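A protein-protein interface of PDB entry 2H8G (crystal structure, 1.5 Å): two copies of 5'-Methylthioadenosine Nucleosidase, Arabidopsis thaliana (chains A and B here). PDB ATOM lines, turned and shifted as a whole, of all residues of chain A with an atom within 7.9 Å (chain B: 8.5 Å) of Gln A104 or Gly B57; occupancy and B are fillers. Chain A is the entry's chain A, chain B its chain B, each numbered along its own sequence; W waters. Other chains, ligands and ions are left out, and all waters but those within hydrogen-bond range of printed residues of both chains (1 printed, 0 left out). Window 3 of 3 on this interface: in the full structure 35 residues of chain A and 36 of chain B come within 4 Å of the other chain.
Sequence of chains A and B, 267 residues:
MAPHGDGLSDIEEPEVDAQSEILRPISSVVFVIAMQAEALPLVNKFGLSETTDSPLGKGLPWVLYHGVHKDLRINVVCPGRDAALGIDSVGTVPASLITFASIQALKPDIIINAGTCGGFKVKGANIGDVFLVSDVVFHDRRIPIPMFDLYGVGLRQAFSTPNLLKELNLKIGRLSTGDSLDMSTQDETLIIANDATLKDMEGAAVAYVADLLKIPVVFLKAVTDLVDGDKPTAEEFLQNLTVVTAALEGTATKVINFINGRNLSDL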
ATOM      1  N   LEU A  56       7.831 -39.522   2.786  1.00  0.00           N
ATOM      2  CA  LEU A  56       6.814 -38.657   3.368  1.00  0.00           C
ATOM      3  C   LEU A  56       5.907 -39.329   4.393  1.00  0.00           C
ATOM      4  O   LEU A  56       5.918 -38.963   5.569  1.00  0.00           O
ATOM      5  CB  LEU A  56       5.970 -38.038   2.251  1.00  0.00           C
ATOM      6  CG  LEU A  56       5.022 -36.918   2.678  1.00  0.00           C
ATOM      7  CD1 LEU A  56       5.781 -35.904   3.518  1.00  0.00           C
ATOM      8  CD2 LEU A  56       4.423 -36.256   1.446  1.00  0.00           C
ATOM      9  N   LEU A  97      -2.985 -31.550   1.251  1.00  0.00           N
ATOM     10  CA  LEU A  97      -2.337 -32.519   2.135  1.00  0.00           C
ATOM     11  C   LEU A  97      -0.905 -32.839   1.719  1.00  0.00           C
ATOM     12  O   LEU A  97       0.000 -32.831   2.556  1.00  0.00           O
ATOM     13  CB  LEU A  97      -3.152 -33.812   2.201  1.00  0.00           C
ATOM     14  CG  LEU A  97      -4.538 -33.705   2.836  1.00  0.00           C
ATOM     15  CD1 LEU A  97      -5.318 -34.976   2.571  1.00  0.00           C
ATOM     16  CD2 LEU A  97      -4.398 -33.454   4.329  1.00  0.00           C
ATOM     17  N   ILE A  98      -0.681 -33.115   0.437  1.00  0.00           N
ATOM     18  CA  ILE A  98       0.678 -33.433   0.011  1.00  0.00           C
ATOM     19  C   ILE A  98       1.588 -32.212   0.065  1.00  0.00           C
ATOM     20  O   ILE A  98       2.791 -32.338   0.280  1.00  0.00           O
ATOM     21  CB  ILE A  98       0.718 -34.067  -1.403  1.00  0.00           C
ATOM     22  CG1 ILE A  98       0.269 -33.068  -2.470  1.00  0.00           C
ATOM     23  CG2 ILE A  98      -0.162 -35.305  -1.424  1.00  0.00           C
ATOM     24  CD1 ILE A  98       0.355 -33.619  -3.882  1.00  0.00           C
ATOM     25  N   THR A  99       1.022 -31.023  -0.118  1.00  0.00           N
ATOM     26  CA  THR A  99       1.823 -29.809  -0.039  1.00  0.00           C
ATOM     27  C   THR A  99       2.264 -29.630   1.418  1.00  0.00           C
ATOM     28  O   THR A  99       3.433 -29.348   1.694  1.00  0.00           O
ATOM     29  CB  THR A  99       1.021 -28.566  -0.480  1.00  0.00           C
ATOM     30  OG1 THR A  99       0.618 -28.719  -1.844  1.00  0.00           O
ATOM     31  CG2 THR A  99       1.872 -27.312  -0.352  1.00  0.00           C
ATOM     32  N   PHE A 100       1.324 -29.817   2.341  1.00  0.00           N
ATOM     33  CA  PHE A 100       1.608 -29.681   3.762  1.00  0.00           C
ATOM     34  C   PHE A 100       2.653 -30.701   4.213  1.00  0.00           C
ATOM     35  O   PHE A 100       3.656 -30.341   4.827  1.00  0.00           O
ATOM     36  CB  PHE A 100       0.326 -29.879   4.575  1.00  0.00           C
ATOM     37  CG  PHE A 100       0.537 -29.839   6.062  1.00  0.00           C
ATOM     38  CD1 PHE A 100       0.751 -28.631   6.718  1.00  0.00           C
ATOM     39  CD2 PHE A 100       0.543 -31.015   6.804  1.00  0.00           C
ATOM     40  CE1 PHE A 100       0.970 -28.597   8.097  1.00  0.00           C
ATOM     41  CE2 PHE A 100       0.761 -30.991   8.180  1.00  0.00           C
ATOM     42  CZ  PHE A 100       0.974 -29.781   8.824  1.00  0.00           C
ATOM     43  N   ALA A 101       2.420 -31.972   3.899  1.00  0.00           N
ATOM     44  CA  ALA A 101       3.346 -33.028   4.303  1.00  0.00           C
ATOM     45  C   ALA A 101       4.726 -32.881   3.662  1.00  0.00           C
ATOM     46  O   ALA A 101       5.747 -33.106   4.318  1.00  0.00           O
ATOM     47  CB  ALA A 101       2.748 -34.396   3.974  1.00  0.00           C
ATOM     48  N   SER A 102       4.754 -32.500   2.388  1.00  0.00           N
ATOM     49  CA  SER A 102       6.010 -32.319   1.663  1.00  0.00           C
ATOM     50  C   SER A 102       6.840 -31.184   2.251  1.00  0.00           C
ATOM     51  O   SER A 102       8.068 -31.286   2.342  1.00  0.00           O
ATOM     52  CB  SER A 102       5.729 -32.038   0.184  1.00  0.00           C
ATOM     53  OG  SER A 102       5.070 -33.142  -0.407  1.00  0.00           O
ATOM     54  N   ILE A 103       6.177 -30.100   2.644  1.00  0.00           N
ATOM     55  CA  ILE A 103       6.880 -28.964   3.227  1.00  0.00           C
ATOM     56  C   ILE A 103       7.512 -29.349   4.561  1.00  0.00           C
ATOM     57  O   ILE A 103       8.679 -29.048   4.812  1.00  0.00           O
ATOM     58  CB  ILE A 103       5.931 -27.770   3.466  1.00  0.00           C
ATOM     59  CG1 ILE A 103       5.517 -27.163   2.123  1.00  0.00           C
ATOM     60  CG2 ILE A 103       6.619 -26.713   4.340  1.00  0.00           C
ATOM     61  CD1 ILE A 103       4.475 -26.066   2.241  1.00  0.00           C
ATOM     62  N   GLN A 104       6.743 -30.019   5.412  1.00  0.00           N
ATOM     63  CA  GLN A 104       7.249 -30.412   6.726  1.00  0.00           C
ATOM     64  C   GLN A 104       8.344 -31.472   6.683  1.00  0.00           C
ATOM     65  O   GLN A 104       9.253 -31.466   7.515  1.00  0.00           O
ATOM     66  CB  GLN A 104       6.094 -30.883   7.617  1.00  0.00           C
ATOM     67  CG  GLN A 104       5.200 -29.736   8.066  1.00  0.00           C
ATOM     68  CD  GLN A 104       4.299 -30.094   9.228  1.00  0.00           C
ATOM     69  OE1 GLN A 104       3.882 -29.219   9.993  1.00  0.00           O
ATOM     70  NE2 GLN A 104       3.985 -31.376   9.367  1.00  0.00           N
ATOM     71  N   ALA A 105       8.274 -32.372   5.711  1.00  0.00           N
ATOM     72  CA  ALA A 105       9.273 -33.427   5.602  1.00  0.00           C
ATOM     73  C   ALA A 105      10.480 -33.060   4.744  1.00  0.00           C
ATOM     74  O   ALA A 105      11.620 -33.365   5.107  1.00  0.00           O
ATOM     75  CB  ALA A 105       8.631 -34.692   5.062  1.00  0.00           C
ATOM     76  N   LEU A 106      10.235 -32.392   3.620  1.00  0.00           N
ATOM     77  CA  LEU A 106      11.302 -32.033   2.690  1.00  0.00           C
ATOM     78  C   LEU A 106      11.912 -30.639   2.858  1.00  0.00           C
ATOM     79  O   LEU A 106      12.993 -30.370   2.334  1.00  0.00           O
ATOM     80  CB  LEU A 106      10.795 -32.213   1.254  1.00  0.00           C
ATOM     81  CG  LEU A 106      10.116 -33.563   0.984  1.00  0.00           C
ATOM     82  CD1 LEU A 106       9.694 -33.647  -0.475  1.00  0.00           C
ATOM     83  CD2 LEU A 106      11.065 -34.706   1.334  1.00  0.00           C
ATOM     84  N   LYS A 107      11.220 -29.759   3.576  1.00  0.00           N
ATOM     85  CA  LYS A 107      11.697 -28.399   3.827  1.00  0.00           C
ATOM     86  C   LYS A 107      12.301 -27.737   2.586  1.00  0.00           C
ATOM     87  O   LYS A 107      13.464 -27.324   2.579  1.00  0.00           O
ATOM     88  CB  LYS A 107      12.719 -28.426   4.967  1.00  0.00           C
ATOM     89  CG  LYS A 107      12.222 -29.211   6.176  1.00  0.00           C
ATOM     90  CD  LYS A 107      13.254 -29.277   7.284  1.00  0.00           C
ATOM     91  CE  LYS A 107      12.857 -30.309   8.331  1.00  0.00           C
ATOM     92  NZ  LYS A 107      12.871 -31.692   7.768  1.00  0.00           N
ATOM     93  N   PRO A 108      11.506 -27.615   1.515  1.00  0.00           N
ATOM     94  CA  PRO A 108      11.963 -27.003   0.265  1.00  0.00           C
ATOM     95  C   PRO A 108      12.154 -25.494   0.388  1.00  0.00           C
ATOM     96  O   PRO A 108      11.609 -24.858   1.290  1.00  0.00           O
ATOM     97  CB  PRO A 108      10.843 -27.361  -0.710  1.00  0.00           C
ATOM     98  CG  PRO A 108       9.638 -27.294   0.159  1.00  0.00           C
ATOM     99  CD  PRO A 108      10.092 -28.018   1.416  1.00  0.00           C
ATOM    100  N   VAL A 209      -1.695 -23.492   1.641  1.00  0.00           N
ATOM    101  CA  VAL A 209      -0.755 -24.201   2.502  1.00  0.00           C
ATOM    102  C   VAL A 209       0.630 -23.569   2.479  1.00  0.00           C
ATOM    103  O   VAL A 209       1.270 -23.430   3.525  1.00  0.00           O
ATOM    104  CB  VAL A 209      -0.639 -25.683   2.084  1.00  0.00           C
ATOM    105  CG1 VAL A 209       0.413 -26.394   2.939  1.00  0.00           C
ATOM    106  CG2 VAL A 209      -1.988 -26.356   2.231  1.00  0.00           C
ATOM    107  N   LEU A 213       2.719 -22.006   5.808  1.00  0.00           N
ATOM    108  CA  LEU A 213       4.057 -22.412   6.214  1.00  0.00           C
ATOM    109  C   LEU A 213       5.161 -21.508   5.683  1.00  0.00           C
ATOM    110  O   LEU A 213       6.345 -21.849   5.746  1.00  0.00           O
ATOM    111  CB  LEU A 213       4.293 -23.867   5.799  1.00  0.00           C
ATOM    112  CG  LEU A 213       3.368 -24.854   6.521  1.00  0.00           C
ATOM    113  CD1 LEU A 213       3.589 -26.258   5.991  1.00  0.00           C
ATOM    114  CD2 LEU A 213       3.631 -24.794   8.025  1.00  0.00           C
ATOM    115  N   ILE A 215       6.257 -20.629   2.661  1.00  0.00           N
ATOM    116  CA  ILE A 215       7.147 -21.165   1.637  1.00  0.00           C
ATOM    117  C   ILE A 215       6.765 -20.525   0.306  1.00  0.00           C
ATOM    118  O   ILE A 215       5.598 -20.540  -0.076  1.00  0.00           O
ATOM    119  CB  ILE A 215       6.998 -22.698   1.491  1.00  0.00           C
ATOM    120  CG1 ILE A 215       7.250 -23.383   2.837  1.00  0.00           C
ATOM    121  CG2 ILE A 215       7.978 -23.222   0.440  1.00  0.00           C
ATOM    122  CD1 ILE A 215       8.625 -23.119   3.415  1.00  0.00           C
ATOM    123  N   ASP B  53       2.962 -25.915  22.887  1.00  0.00           N
ATOM    124  CA  ASP B  53       4.174 -26.298  22.175  1.00  0.00           C
ATOM    125  C   ASP B  53       4.030 -26.572  20.679  1.00  0.00           C
ATOM    126  O   ASP B  53       4.834 -27.302  20.098  1.00  0.00           O
ATOM    127  CB  ASP B  53       4.824 -27.500  22.876  1.00  0.00           C
ATOM    128  CG  ASP B  53       3.982 -28.757  22.797  1.00  0.00           C
ATOM    129  OD1 ASP B  53       2.736 -28.652  22.805  1.00  0.00           O
ATOM    130  OD2 ASP B  53       4.569 -29.857  22.745  1.00  0.00           O
ATOM    131  N   SER B  54       3.014 -25.971  20.061  1.00  0.00           N
ATOM    132  CA  SER B  54       2.761 -26.111  18.625  1.00  0.00           C
ATOM    133  C   SER B  54       3.105 -27.495  18.077  1.00  0.00           C
ATOM    134  O   SER B  54       3.890 -27.615  17.138  1.00  0.00           O
ATOM    135  CB  SER B  54       3.566 -25.058  17.859  1.00  0.00           C
ATOM    136  OG  SER B  54       3.300 -23.754  18.347  1.00  0.00           O
ATOM    137  N   PRO B  55       2.492 -28.554  18.631  1.00  0.00           N
ATOM    138  CA  PRO B  55       2.732 -29.940  18.213  1.00  0.00           C
ATOM    139  C   PRO B  55       2.390 -30.310  16.773  1.00  0.00           C
ATOM    140  O   PRO B  55       2.883 -31.313  16.256  1.00  0.00           O
ATOM    141  CB  PRO B  55       1.908 -30.744  19.215  1.00  0.00           C
ATOM    142  CG  PRO B  55       0.762 -29.850  19.482  1.00  0.00           C
ATOM    143  CD  PRO B  55       1.421 -28.500  19.643  1.00  0.00           C
ATOM    144  N   LEU B  56       1.550 -29.516  16.121  1.00  0.00           N
ATOM    145  CA  LEU B  56       1.171 -29.817  14.748  1.00  0.00           C
ATOM    146  C   LEU B  56       2.053 -29.091  13.741  1.00  0.00           C
ATOM    147  O   LEU B  56       1.992 -29.359  12.542  1.00  0.00           O
ATOM    148  CB  LEU B  56      -0.299 -29.451  14.525  1.00  0.00           C
ATOM    149  CG  LEU B  56      -1.266 -30.085  15.531  1.00  0.00           C
ATOM    150  CD1 LEU B  56      -2.688 -29.674  15.191  1.00  0.00           C
ATOM    151  CD2 LEU B  56      -1.123 -31.602  15.512  1.00  0.00           C
ATOM    152  N   GLY B  57       2.879 -28.175  14.235  1.00  0.00           N
ATOM    153  CA  GLY B  57       3.757 -27.425  13.358  1.00  0.00           C
ATOM    154  C   GLY B  57       3.939 -26.009  13.860  1.00  0.00           C
ATOM    155  O   GLY B  57       3.028 -25.430  14.449  1.00  0.00           O
ATOM    156  N   LYS B  58       5.114 -25.439  13.623  1.00  0.00           N
ATOM    157  CA  LYS B  58       5.391 -24.087  14.079  1.00  0.00           C
ATOM    158  C   LYS B  58       4.815 -23.029  13.143  1.00  0.00           C
ATOM    159  O   LYS B  58       4.745 -23.223  11.928  1.00  0.00           O
ATOM    160  CB  LYS B  58       6.902 -23.884  14.224  1.00  0.00           C
ATOM    161  CG  LYS B  58       7.283 -22.607  14.950  1.00  0.00           C
ATOM    162  CD  LYS B  58       8.780 -22.534  15.206  1.00  0.00           C
ATOM    163  CE  LYS B  58       9.130 -21.303  16.028  1.00  0.00           C
ATOM    164  NZ  LYS B  58      10.586 -21.222  16.327  1.00  0.00           N
ATOM    165  N   GLY B  59       4.390 -21.914  13.728  1.00  0.00           N
ATOM    166  CA  GLY B  59       3.842 -20.817  12.952  1.00  0.00           C
ATOM    167  C   GLY B  59       2.434 -20.994  12.413  1.00  0.00           C
ATOM    168  O   GLY B  59       1.951 -20.149  11.659  1.00  0.00           O
ATOM    169  N   LEU B  60       1.764 -22.074  12.800  1.00  0.00           N
ATOM    170  CA  LEU B  60       0.410 -22.334  12.324  1.00  0.00           C
ATOM    171  C   LEU B  60      -0.645 -21.702  13.229  1.00  0.00           C
ATOM    172  O   LEU B  60      -0.452 -21.595  14.440  1.00  0.00           O
ATOM    173  CB  LEU B  60       0.178 -23.842  12.223  1.00  0.00           C
ATOM    174  CG  LEU B  60       1.073 -24.581  11.224  1.00  0.00           C
ATOM    175  CD1 LEU B  60       0.915 -26.073  11.419  1.00  0.00           C
ATOM    176  CD2 LEU B  60       0.709 -24.180   9.797  1.00  0.00           C
ATOM    177  N   PRO B  61      -1.783 -21.283  12.649  1.00  0.00           N
ATOM    178  CA  PRO B  61      -2.875 -20.656  13.399  1.00  0.00           C
ATOM    179  C   PRO B  61      -3.760 -21.665  14.123  1.00  0.00           C
ATOM    180  O   PRO B  61      -4.626 -21.289  14.912  1.00  0.00           O
ATOM    181  CB  PRO B  61      -3.640 -19.910  12.316  1.00  0.00           C
ATOM    182  CG  PRO B  61      -3.537 -20.855  11.160  1.00  0.00           C
ATOM    183  CD  PRO B  61      -2.080 -21.286  11.203  1.00  0.00           C
ATOM    184  N   TRP B  62      -3.534 -22.943  13.844  1.00  0.00           N
ATOM    185  CA  TRP B  62      -4.318 -24.015  14.446  1.00  0.00           C
ATOM    186  C   TRP B  62      -4.281 -23.980  15.968  1.00  0.00           C
ATOM    187  O   TRP B  62      -3.257 -23.649  16.578  1.00  0.00           O
ATOM    188  CB  TRP B  62      -3.817 -25.368  13.938  1.00  0.00           C
ATOM    189  CG  TRP B  62      -3.785 -25.457  12.441  1.00  0.00           C
ATOM    190  CD1 TRP B  62      -4.430 -24.638  11.558  1.00  0.00           C
ATOM    191  CD2 TRP B  62      -3.105 -26.440  11.651  1.00  0.00           C
ATOM    192  NE1 TRP B  62      -4.196 -25.050  10.269  1.00  0.00           N
ATOM    193  CE2 TRP B  62      -3.386 -26.154  10.296  1.00  0.00           C
ATOM    194  CE3 TRP B  62      -2.287 -27.536  11.956  1.00  0.00           C
ATOM    195  CZ2 TRP B  62      -2.879 -26.927   9.244  1.00  0.00           C
ATOM    196  CZ3 TRP B  62      -1.782 -28.306  10.909  1.00  0.00           C
ATOM    197  CH2 TRP B  62      -2.082 -27.995   9.569  1.00  0.00           C
ATOM    198  N   LEU B  64      -5.047 -26.211  19.474  1.00  0.00           N
ATOM    199  CA  LEU B  64      -5.249 -27.547  20.014  1.00  0.00           C
ATOM    200  C   LEU B  64      -5.497 -27.462  21.513  1.00  0.00           C
ATOM    201  O   LEU B  64      -4.678 -26.916  22.253  1.00  0.00           O
ATOM    202  CB  LEU B  64      -4.016 -28.423  19.743  1.00  0.00           C
ATOM    203  CG  LEU B  64      -4.081 -29.901  20.153  1.00  0.00           C
ATOM    204  CD1 LEU B  64      -5.173 -30.614  19.363  1.00  0.00           C
ATOM    205  CD2 LEU B  64      -2.737 -30.560  19.895  1.00  0.00           C
ATOM    206  N   LEU B  97      -6.507 -30.659   6.648  1.00  0.00           N
ATOM    207  CA  LEU B  97      -5.160 -30.456   7.166  1.00  0.00           C
ATOM    208  C   LEU B  97      -5.041 -30.747   8.652  1.00  0.00           C
ATOM    209  O   LEU B  97      -4.136 -31.471   9.072  1.00  0.00           O
ATOM    210  CB  LEU B  97      -4.702 -29.017   6.894  1.00  0.00           C
ATOM    211  CG  LEU B  97      -4.439 -28.659   5.427  1.00  0.00           C
ATOM    212  CD1 LEU B  97      -4.309 -27.155   5.271  1.00  0.00           C
ATOM    213  CD2 LEU B  97      -3.173 -29.359   4.955  1.00  0.00           C
ATOM    214  N   PHE B 100      -5.441 -34.455   9.358  1.00  0.00           N
ATOM    215  CA  PHE B 100      -4.223 -35.160   8.999  1.00  0.00           C
ATOM    216  C   PHE B 100      -3.135 -34.958  10.049  1.00  0.00           C
ATOM    217  O   PHE B 100      -2.560 -35.920  10.563  1.00  0.00           O
ATOM    218  CB  PHE B 100      -3.712 -34.654   7.646  1.00  0.00           C
ATOM    219  CG  PHE B 100      -2.405 -35.264   7.223  1.00  0.00           C
ATOM    220  CD1 PHE B 100      -2.373 -36.514   6.619  1.00  0.00           C
ATOM    221  CD2 PHE B 100      -1.206 -34.588   7.436  1.00  0.00           C
ATOM    222  CE1 PHE B 100      -1.167 -37.085   6.229  1.00  0.00           C
ATOM    223  CE2 PHE B 100       0.009 -35.150   7.049  1.00  0.00           C
ATOM    224  CZ  PHE B 100       0.027 -36.400   6.445  1.00  0.00           C
ATOM    225  N   ALA B 101      -2.863 -33.700  10.371  1.00  0.00           N
ATOM    226  CA  ALA B 101      -1.820 -33.371  11.329  1.00  0.00           C
ATOM    227  C   ALA B 101      -2.088 -33.916  12.722  1.00  0.00           C
ATOM    228  O   ALA B 101      -1.180 -34.435  13.377  1.00  0.00           O
ATOM    229  CB  ALA B 101      -1.626 -31.864  11.379  1.00  0.00           C
ATOM    230  N   SER B 102      -3.329 -33.818  13.183  1.00  0.00           N
ATOM    231  CA  SER B 102      -3.645 -34.303  14.519  1.00  0.00           C
ATOM    232  C   SER B 102      -3.579 -35.826  14.612  1.00  0.00           C
ATOM    233  O   SER B 102      -3.187 -36.363  15.649  1.00  0.00           O
ATOM    234  CB  SER B 102      -5.017 -33.787  14.974  1.00  0.00           C
ATOM    235  OG  SER B 102      -6.067 -34.301  14.179  1.00  0.00           O
ATOM    236  N   GLN B 104      -1.578 -37.863  12.781  1.00  0.00           N
ATOM    237  CA  GLN B 104      -0.171 -38.257  12.753  1.00  0.00           C
ATOM    238  C   GLN B 104       0.547 -37.959  14.060  1.00  0.00           C
ATOM    239  O   GLN B 104       1.426 -38.715  14.483  1.00  0.00           O
ATOM    240  CB  GLN B 104       0.554 -37.568  11.591  1.00  0.00           C
ATOM    241  CG  GLN B 104       0.497 -36.044  11.609  1.00  0.00           C
ATOM    242  CD  GLN B 104       1.548 -35.406  12.508  1.00  0.00           C
ATOM    243  OE1 GLN B 104       1.570 -34.185  12.683  1.00  0.00           O
ATOM    244  NE2 GLN B 104       2.429 -36.227  13.074  1.00  0.00           N
ATOM    245  N   ALA B 105       0.167 -36.864  14.708  1.00  0.00           N
ATOM    246  CA  ALA B 105       0.800 -36.464  15.958  1.00  0.00           C
ATOM    247  C   ALA B 105       0.237 -37.150  17.198  1.00  0.00           C
ATOM    248  O   ALA B 105       0.996 -37.577  18.077  1.00  0.00           O
ATOM    249  CB  ALA B 105       0.701 -34.955  16.120  1.00  0.00           C
HETATM  250  O   HOH W   1       2.009 -31.796  11.507  1.00  0.00           O
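O of Leu B56 lies close to OE1 of Gln A104 (3.2 Å).
Water W1 lies within hydrogen-bond range of O of Leu B56 (2.6 Å), OE1 of Gln B104 (2.7 Å) and NE2 of Gln A104 (2.9 Å).
Of chain B, only Leu B56 (3.2 Å) and Gly B57 (3.8 Å) come within 4 Å of Gln A104. No residue of chain B comes within 4 Å of Ala A105. Printed residues of chain A within 4 Å of Phe B100: Leu A97 (3.6 Å). Printed residues of chain A within 4 Å of Leu B56: Phe A100 (3.9 Å) and Gln A104 (3.2 Å). Ile A103 touches none of the printed residues of chain B. Ala B105 touches none of the printed residues of chain A. The nearest residue of chain B that does not touch Gln A104 is Leu B60 (4.6 Å). The nearest printed residue of chain B that does not touch Leu A97 is Leu B97 (4.2 Å).
Leu A97 touches Phe B100, and with the chains exchanged Phe A100 touches Leu B97. Phe A100 touches Leu B56, but with the chains exchanged Leu A56 does not touch Phe B100 (6.3 Å). Gln A104 touches Leu B56, but with the chains exchanged Leu A56 does not touch Gln B104 (8.2 Å). Positions printed for both chains: 56, 97, 100, 101, 102, 104 and 105. Of the 8 pairs that touch across the chains among the printed residues, 2 have their exchanged pair printed and touching as well.
Among the printed residues, pairs that only touch across the chains: Leu A97 with Phe B100 (3.6 Å), Phe A100 with Leu B56 (3.9 Å), Phe A100 with Trp B62 (3.4 Å), Phe A100 with Leu B97 (3.6 Å), Gln A104 with Gly B57 (3.8 Å), Val A209 with Leu B97 (3.9 Å) and Leu A213 with Leu B60 (3.5 Å).
Of the 16 printed residues of chain A, 5 touch a printed residue of chain B. Printed residues of chain A that touch a printed residue of chain B: Leu A97, Phe A100, Gln A104, Val A209 and Leu A213. Of the 17 printed residues of chain B, 6 touch a printed residue of chain A. Hydrophobic or aromatic side chains of chain B within 4 Å of the printed part of chain A: Leu B60, Trp B62, Leu B97 and Phe B100.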
